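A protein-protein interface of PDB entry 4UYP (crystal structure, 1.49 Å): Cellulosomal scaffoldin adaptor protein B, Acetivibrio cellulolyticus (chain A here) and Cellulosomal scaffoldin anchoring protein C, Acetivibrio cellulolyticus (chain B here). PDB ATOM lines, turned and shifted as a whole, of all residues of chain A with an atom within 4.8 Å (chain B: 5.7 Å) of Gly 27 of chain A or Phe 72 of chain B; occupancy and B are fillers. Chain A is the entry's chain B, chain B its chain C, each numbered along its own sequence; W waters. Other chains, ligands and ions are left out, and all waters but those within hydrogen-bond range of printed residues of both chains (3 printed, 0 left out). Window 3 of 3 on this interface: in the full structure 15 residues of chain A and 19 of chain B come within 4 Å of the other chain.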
ATOM      1  N   ASP A  23      -7.562  19.307  -0.260  1.00  0.00           N
ATOM      2  CA  ASP A  23      -8.188  18.773   1.003  1.00  0.00           C
ATOM      3  C   ASP A  23      -7.622  17.417   1.233  1.00  0.00           C
ATOM      4  O   ASP A  23      -7.401  17.031   2.425  1.00  0.00           O
ATOM      5  CB  ASP A  23      -9.708  18.673   0.847  1.00  0.00           C
ATOM      6  CG  ASP A  23     -10.411  19.963   0.971  1.00  0.00           C
ATOM      7  OD1 ASP A  23      -9.835  20.980   1.359  1.00  0.00           O
ATOM      8  OD2 ASP A  23     -11.661  19.848   0.577  1.00  0.00           O
ATOM      9  N   TYR A  24      -7.430  16.552   0.202  1.00  0.00           N
ATOM     10  CA  TYR A  24      -6.845  15.248   0.434  1.00  0.00           C
ATOM     11  C   TYR A  24      -5.401  15.283   0.942  1.00  0.00           C
ATOM     12  O   TYR A  24      -4.998  14.570   1.893  1.00  0.00           O
ATOM     13  CB  TYR A  24      -6.891  14.440  -0.916  1.00  0.00           C
ATOM     14  CG  TYR A  24      -6.541  13.007  -0.807  1.00  0.00           C
ATOM     15  CD1 TYR A  24      -5.210  12.566  -0.885  1.00  0.00           C
ATOM     16  CD2 TYR A  24      -7.577  12.050  -0.572  1.00  0.00           C
ATOM     17  CE1 TYR A  24      -4.873  11.221  -0.730  1.00  0.00           C
ATOM     18  CE2 TYR A  24      -7.203  10.717  -0.523  1.00  0.00           C
ATOM     19  CZ  TYR A  24      -5.879  10.318  -0.540  1.00  0.00           C
ATOM     20  OH  TYR A  24      -5.609   8.947  -0.403  1.00  0.00           O
ATOM     21  N   VAL A  25      -4.575  16.153   0.303  1.00  0.00           N
ATOM     22  CA  VAL A  25      -3.221  16.317   0.747  1.00  0.00           C
ATOM     23  C   VAL A  25      -3.129  16.811   2.209  1.00  0.00           C
ATOM     24  O   VAL A  25      -2.250  16.348   2.979  1.00  0.00           O
ATOM     25  CB  VAL A  25      -2.499  17.247  -0.260  1.00  0.00           C
ATOM     26  CG1 VAL A  25      -1.083  17.483   0.268  1.00  0.00           C
ATOM     27  CG2 VAL A  25      -2.428  16.607  -1.642  1.00  0.00           C
ATOM     28  N   LEU A  26      -4.012  17.735   2.548  1.00  0.00           N
ATOM     29  CA  LEU A  26      -4.094  18.290   3.930  1.00  0.00           C
ATOM     30  C   LEU A  26      -4.556  17.259   4.937  1.00  0.00           C
ATOM     31  O   LEU A  26      -4.362  17.449   6.158  1.00  0.00           O
ATOM     32  CB  LEU A  26      -5.004  19.489   3.948  1.00  0.00           C
ATOM     33  CG  LEU A  26      -4.490  20.832   3.330  1.00  0.00           C
ATOM     34  CD1 LEU A  26      -5.635  21.801   3.117  1.00  0.00           C
ATOM     35  CD2 LEU A  26      -3.375  21.417   4.175  1.00  0.00           C
ATOM     36  N   GLY A  27      -5.230  16.218   4.469  1.00  0.00           N
ATOM     37  CA  GLY A  27      -5.785  15.228   5.417  1.00  0.00           C
ATOM     38  C   GLY A  27      -7.180  15.560   5.852  1.00  0.00           C
ATOM     39  O   GLY A  27      -7.690  14.854   6.755  1.00  0.00           O
ATOM     40  N   LYS A  28      -7.859  16.562   5.305  1.00  0.00           N
ATOM     41  CA  LYS A  28      -9.240  16.861   5.651  1.00  0.00           C
ATOM     42  C   LYS A  28     -10.183  15.763   5.139  1.00  0.00           C
ATOM     43  O   LYS A  28     -11.234  15.505   5.769  1.00  0.00           O
ATOM     44  CB  LYS A  28      -9.521  18.163   4.988  1.00  0.00           C
ATOM     45  CG  LYS A  28     -10.854  18.705   5.337  1.00  0.00           C
ATOM     46  CD  LYS A  28     -11.031  20.112   4.859  1.00  0.00           C
ATOM     47  CE  LYS A  28     -12.455  20.562   5.089  1.00  0.00           C
ATOM     48  NZ  LYS A  28     -12.339  22.035   5.218  1.00  0.00           N
ATOM     49  N   ILE A  29      -9.782  15.075   4.071  1.00  0.00           N
ATOM     50  CA  ILE A  29     -10.503  13.937   3.552  1.00  0.00           C
ATOM     51  C   ILE A  29      -9.572  12.827   3.365  1.00  0.00           C
ATOM     52  O   ILE A  29      -8.398  13.047   3.069  1.00  0.00           O
ATOM     53  CB  ILE A  29     -11.301  14.293   2.242  1.00  0.00           C
ATOM     54  CG1 ILE A  29     -10.389  14.723   1.047  1.00  0.00           C
ATOM     55  CG2 ILE A  29     -12.320  15.377   2.483  1.00  0.00           C
ATOM     56  CD1 ILE A  29     -11.170  15.250  -0.199  1.00  0.00           C
ATOM     57  N   ASN A  30     -10.093  11.575   3.358  1.00  0.00           N
ATOM     58  CA  ASN A  30      -9.300  10.380   3.174  1.00  0.00           C
ATOM     59  C   ASN A  30      -9.678   9.607   1.885  1.00  0.00           C
ATOM     60  O   ASN A  30      -9.036   8.625   1.528  1.00  0.00           O
ATOM     61  CB  ASN A  30      -9.616   9.430   4.379  1.00  0.00           C
ATOM     62  CG  ASN A  30      -9.006   9.949   5.655  1.00  0.00           C
ATOM     63  OD1 ASN A  30      -7.890  10.435   5.570  1.00  0.00           O
ATOM     64  ND2 ASN A  30      -9.739   9.993   6.734  1.00  0.00           N
ATOM     65  N   ARG B  37       3.596  18.263   6.546  1.00  0.00           N
ATOM     66  CA  ARG B  37       2.759  17.723   7.634  1.00  0.00           C
ATOM     67  C   ARG B  37       3.617  17.311   8.779  1.00  0.00           C
ATOM     68  O   ARG B  37       4.681  16.711   8.583  1.00  0.00           O
ATOM     69  CB  ARG B  37       2.061  16.493   7.079  1.00  0.00           C
ATOM     70  CG  ARG B  37       1.184  15.909   8.202  1.00  0.00           C
ATOM     71  CD  ARG B  37       0.324  14.714   7.787  1.00  0.00           C
ATOM     72  NE  ARG B  37      -0.604  15.120   6.772  1.00  0.00           N
ATOM     73  CZ  ARG B  37      -1.607  14.344   6.446  1.00  0.00           C
ATOM     74  NH1 ARG B  37      -1.854  13.146   7.000  1.00  0.00           N
ATOM     75  NH2 ARG B  37      -2.473  14.721   5.505  1.00  0.00           N
ATOM     76  N   THR B  38       3.179  17.697   9.972  1.00  0.00           N
ATOM     77  CA  THR B  38       3.837  17.309  11.264  1.00  0.00           C
ATOM     78  C   THR B  38       2.905  16.393  11.997  1.00  0.00           C
ATOM     79  O   THR B  38       1.698  16.639  12.090  1.00  0.00           O
ATOM     80  CB  THR B  38       4.040  18.523  12.244  1.00  0.00           C
ATOM     81  OG1 THR B  38       2.806  19.129  12.561  1.00  0.00           O
ATOM     82  CG2 THR B  38       4.994  19.582  11.568  1.00  0.00           C
ATOM     83  N   ASN B  39       3.448  15.323  12.626  1.00  0.00           N
ATOM     84  CA  ASN B  39       2.674  14.582  13.627  1.00  0.00           C
ATOM     85  C   ASN B  39       3.138  14.890  15.060  1.00  0.00           C
ATOM     86  O   ASN B  39       4.237  15.350  15.278  1.00  0.00           O
ATOM     87  CB  ASN B  39       2.863  13.048  13.357  1.00  0.00           C
ATOM     88  CG  ASN B  39       2.163  12.634  12.023  1.00  0.00           C
ATOM     89  OD1 ASN B  39       2.891  12.483  10.998  1.00  0.00           O
ATOM     90  ND2 ASN B  39       0.876  12.516  12.020  1.00  0.00           N
ATOM     91  N   PHE B  40       2.204  14.513  15.886  1.00  0.00           N
ATOM     92  CA  PHE B  40       2.417  14.677  17.350  1.00  0.00           C
ATOM     93  C   PHE B  40       1.472  13.725  18.063  1.00  0.00           C
ATOM     94  O   PHE B  40       0.460  13.264  17.531  1.00  0.00           O
ATOM     95  CB  PHE B  40       2.095  16.133  17.799  1.00  0.00           C
ATOM     96  CG  PHE B  40       0.690  16.613  17.398  1.00  0.00           C
ATOM     97  CD1 PHE B  40       0.506  17.234  16.087  1.00  0.00           C
ATOM     98  CD2 PHE B  40      -0.476  16.479  18.256  1.00  0.00           C
ATOM     99  CE1 PHE B  40      -0.775  17.706  15.725  1.00  0.00           C
ATOM    100  CE2 PHE B  40      -1.724  16.954  17.867  1.00  0.00           C
ATOM    101  CZ  PHE B  40      -1.877  17.566  16.579  1.00  0.00           C
ATOM    102  N   VAL B  47      -3.115  21.178  18.701  1.00  0.00           N
ATOM    103  CA  VAL B  47      -2.887  22.467  18.023  1.00  0.00           C
ATOM    104  C   VAL B  47      -3.946  23.500  18.421  1.00  0.00           C
ATOM    105  O   VAL B  47      -5.161  23.249  18.292  1.00  0.00           O
ATOM    106  CB  VAL B  47      -2.924  22.299  16.494  1.00  0.00           C
ATOM    107  CG1 VAL B  47      -2.740  23.645  15.760  1.00  0.00           C
ATOM    108  CG2 VAL B  47      -1.830  21.330  16.033  1.00  0.00           C
ATOM    109  N   TYR B  65      -4.581  22.900   8.019  1.00  0.00           N
ATOM    110  CA  TYR B  65      -5.595  21.991   8.545  1.00  0.00           C
ATOM    111  C   TYR B  65      -4.932  21.246   9.674  1.00  0.00           C
ATOM    112  O   TYR B  65      -3.816  20.822   9.552  1.00  0.00           O
ATOM    113  CB  TYR B  65      -6.129  21.019   7.516  1.00  0.00           C
ATOM    114  CG  TYR B  65      -7.130  20.045   8.130  1.00  0.00           C
ATOM    115  CD1 TYR B  65      -8.418  20.483   8.502  1.00  0.00           C
ATOM    116  CD2 TYR B  65      -6.777  18.737   8.277  1.00  0.00           C
ATOM    117  CE1 TYR B  65      -9.285  19.498   9.101  1.00  0.00           C
ATOM    118  CE2 TYR B  65      -7.585  17.805   8.891  1.00  0.00           C
ATOM    119  CZ  TYR B  65      -8.813  18.198   9.227  1.00  0.00           C
ATOM    120  OH  TYR B  65      -9.652  17.260   9.897  1.00  0.00           O
ATOM    121  N   TYR B  66      -5.669  20.945  10.741  1.00  0.00           N
ATOM    122  CA  TYR B  66      -5.105  20.063  11.744  1.00  0.00           C
ATOM    123  C   TYR B  66      -6.227  19.171  12.278  1.00  0.00           C
ATOM    124  O   TYR B  66      -7.379  19.545  12.250  1.00  0.00           O
ATOM    125  CB  TYR B  66      -4.432  20.868  12.876  1.00  0.00           C
ATOM    126  CG  TYR B  66      -5.230  21.953  13.466  1.00  0.00           C
ATOM    127  CD1 TYR B  66      -6.080  21.683  14.506  1.00  0.00           C
ATOM    128  CD2 TYR B  66      -5.121  23.332  13.036  1.00  0.00           C
ATOM    129  CE1 TYR B  66      -6.843  22.663  15.115  1.00  0.00           C
ATOM    130  CE2 TYR B  66      -5.895  24.330  13.711  1.00  0.00           C
ATOM    131  CZ  TYR B  66      -6.767  24.022  14.689  1.00  0.00           C
ATOM    132  OH  TYR B  66      -7.586  24.970  15.307  1.00  0.00           O
ATOM    133  N   ASN B  67      -5.791  18.025  12.764  1.00  0.00           N
ATOM    134  CA  ASN B  67      -6.747  17.078  13.346  1.00  0.00           C
ATOM    135  C   ASN B  67      -6.148  16.689  14.714  1.00  0.00           C
ATOM    136  O   ASN B  67      -5.157  15.970  14.805  1.00  0.00           O
ATOM    137  CB  ASN B  67      -6.859  15.867  12.387  1.00  0.00           C
ATOM    138  CG  ASN B  67      -7.775  14.813  12.896  1.00  0.00           C
ATOM    139  OD1 ASN B  67      -7.931  14.660  14.120  1.00  0.00           O
ATOM    140  ND2 ASN B  67      -8.435  14.039  11.967  1.00  0.00           N
ATOM    141  N   ASN B  68      -6.796  17.169  15.759  1.00  0.00           N
ATOM    142  CA  ASN B  68      -6.309  16.997  17.139  1.00  0.00           C
ATOM    143  C   ASN B  68      -6.759  15.655  17.728  1.00  0.00           C
ATOM    144  O   ASN B  68      -6.334  15.339  18.863  1.00  0.00           O
ATOM    145  CB  ASN B  68      -6.786  18.092  17.982  1.00  0.00           C
ATOM    146  CG  ASN B  68      -5.964  19.404  17.812  1.00  0.00           C
ATOM    147  OD1 ASN B  68      -4.725  19.272  17.583  1.00  0.00           O
ATOM    148  ND2 ASN B  68      -6.549  20.563  17.973  1.00  0.00           N
ATOM    149  N   ASN B  70      -6.352  12.819  15.692  1.00  0.00           N
ATOM    150  CA  ASN B  70      -5.440  11.929  15.044  1.00  0.00           C
ATOM    151  C   ASN B  70      -3.970  12.354  15.116  1.00  0.00           C
ATOM    152  O   ASN B  70      -3.064  11.606  14.835  1.00  0.00           O
ATOM    153  CB  ASN B  70      -5.894  11.743  13.620  1.00  0.00           C
ATOM    154  CG  ASN B  70      -7.212  10.922  13.574  1.00  0.00           C
ATOM    155  OD1 ASN B  70      -7.584  10.310  14.555  1.00  0.00           O
ATOM    156  ND2 ASN B  70      -7.899  10.968  12.468  1.00  0.00           N
ATOM    157  N   GLY B  71      -3.720  13.542  15.546  1.00  0.00           N
ATOM    158  CA  GLY B  71      -2.285  13.896  15.766  1.00  0.00           C
ATOM    159  C   GLY B  71      -1.489  14.364  14.532  1.00  0.00           C
ATOM    160  O   GLY B  71      -0.354  14.009  14.323  1.00  0.00           O
ATOM    161  N   PHE B  72      -2.193  15.231  13.703  1.00  0.00           N
ATOM    162  CA  PHE B  72      -1.335  15.833  12.651  1.00  0.00           C
ATOM    163  C   PHE B  72      -1.832  17.258  12.361  1.00  0.00           C
ATOM    164  O   PHE B  72      -2.930  17.658  12.626  1.00  0.00           O
ATOM    165  CB  PHE B  72      -1.291  15.011  11.327  1.00  0.00           C
ATOM    166  CG  PHE B  72      -2.645  14.928  10.637  1.00  0.00           C
ATOM    167  CD1 PHE B  72      -3.069  15.914   9.676  1.00  0.00           C
ATOM    168  CD2 PHE B  72      -3.536  13.861  10.851  1.00  0.00           C
ATOM    169  CE1 PHE B  72      -4.326  15.785   9.049  1.00  0.00           C
ATOM    170  CE2 PHE B  72      -4.767  13.759  10.172  1.00  0.00           C
ATOM    171  CZ  PHE B  72      -5.214  14.743   9.291  1.00  0.00           C
ATOM    172  N   ALA B  73      -0.873  17.968  11.798  1.00  0.00           N
ATOM    173  CA  ALA B  73      -1.071  19.337  11.276  1.00  0.00           C
ATOM    174  C   ALA B  73      -0.451  19.391   9.915  1.00  0.00           C
ATOM    175  O   ALA B  73       0.694  19.020   9.728  1.00  0.00           O
ATOM    176  CB  ALA B  73      -0.446  20.387  12.186  1.00  0.00           C
ATOM    177  N   SER B  74      -1.190  19.990   8.976  1.00  0.00           N
ATOM    178  CA  SER B  74      -0.770  20.061   7.540  1.00  0.00           C
ATOM    179  C   SER B  74      -0.857  21.489   7.068  1.00  0.00           C
ATOM    180  O   SER B  74      -1.776  22.212   7.430  1.00  0.00           O
ATOM    181  CB  SER B  74      -1.671  19.261   6.604  1.00  0.00           C
ATOM    182  OG  SER B  74      -1.713  17.874   7.012  1.00  0.00           O
HETATM  183  O   HOH W   1       0.149  17.291   4.156  1.00  0.00           O
HETATM  184  O   HOH W   2      -9.996  10.634   9.796  1.00  0.00           O
HETATM  185  O   HOH W   3      -9.119  14.679   9.161  1.00  0.00           O
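NH2 of Arg 37 of chain B sits at hydrogen-bond distance from O of Val 25 of chain A (3.0 Å).
The guanidinium group of Arg 37 of chain B lies close to the backbone carbonyl oxygen of Leu 26 of chain A, 3.4 Å away.
The side-chain hydroxyl (OG) of Ser 74 of chain B is in hydrogen-bond range of the backbone carbonyl oxygen (O) of Leu 26 of chain A, 2.8 Å away.
The backbone NH of Gly 27 of chain A sits close to the guanidinium group of Arg 37 of chain B.
The side-chain hydroxyl (OG) of Ser 74 of chain B lies within hydrogen-bond range of the guanidinium group (NE) of Arg 37 of chain B (3.0 Å).
The backbone carbonyl oxygen (O) of Tyr 65 of chain B sits at hydrogen-bond distance from the backbone NH (N) of Ser 74 of chain B.
N of Asn 67 of chain B is in hydrogen-bond range of O of Phe 72 of chain B, 2.9 Å away.
The backbone carbonyl oxygen (O) of Asp 23 of chain A sits at hydrogen-bond distance from the backbone NH (N) of Lys 28 of chain A, 3.0 Å away.
CD2 of Tyr 65 of chain B touches O of Leu 26 of chain A (3.5 Å).
O of Leu 26 of chain A touches CE1 of Phe 72 of chain B (3.3 Å).
CE2 of Tyr 65 of chain B touches O of Gly 27 of chain A (3.6 Å).
O of Gly 27 of chain A touches CZ of Phe 72 of chain B (3.5 Å).
Tyr 65 of chain B touches Lys 28 of chain A.
Tyr 24 of chain A touches none of the printed residues of chain B.
Of the printed residues of chain B, Val 25 of chain A touches Arg 37.
Of the printed residues of chain B, Leu 26 of chain A touches Arg 37, Tyr 65, Phe 72 and Ser 74.
Of the printed residues of chain B, Gly 27 of chain A touches Arg 37 (3.3 Å), Tyr 65 (3.6 Å) and Phe 72 (3.5 Å).
Of the printed residues of chain B, Lys 28 of chain A touches Tyr 65 (3.8 Å).
Printed residues of chain A within 4 Å of Arg 37 of chain B: Val 25 (3.0 Å), Leu 26 (3.3 Å) and Gly 27 (3.3 Å).
Gly 71 of chain B touches none of the printed residues of chain A.
Of chain A, only Leu 26 (3.3 Å) and Gly 27 (3.5 Å) come within 4 Å of Phe 72 of chain B.
Printed residues of chain A within 4 Å of Ser 74 of chain B: Leu 26.
The nearest printed residue of chain A that does not touch Phe 72 of chain B is Lys 28 of chain A (5.1 Å).
Of the 14 printed residues of chain B, 4 touch a printed residue of chain A.
Hydrophobic or aromatic side chains of chain B within 4 Å of the printed part of chain A: Tyr 65 and Phe 72.
Water W3 lies within hydrogen-bond range of OH of Tyr 65 of chain B, O of Gly 27 of chain A and ND2 of Asn 67 of chain B.
Water W1 lies within hydrogen-bond range of the backbone carbonyl oxygen (O) of Val 25 of chain A, the side-chain hydroxyl (OG) of Ser 74 of chain B and the guanidinium group (NE) of Arg 37 of chain B.
Water W2 lies within hydrogen-bond range of ND2 of Asn 30 of chain A and ND2 of Asn 70 of chain B.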
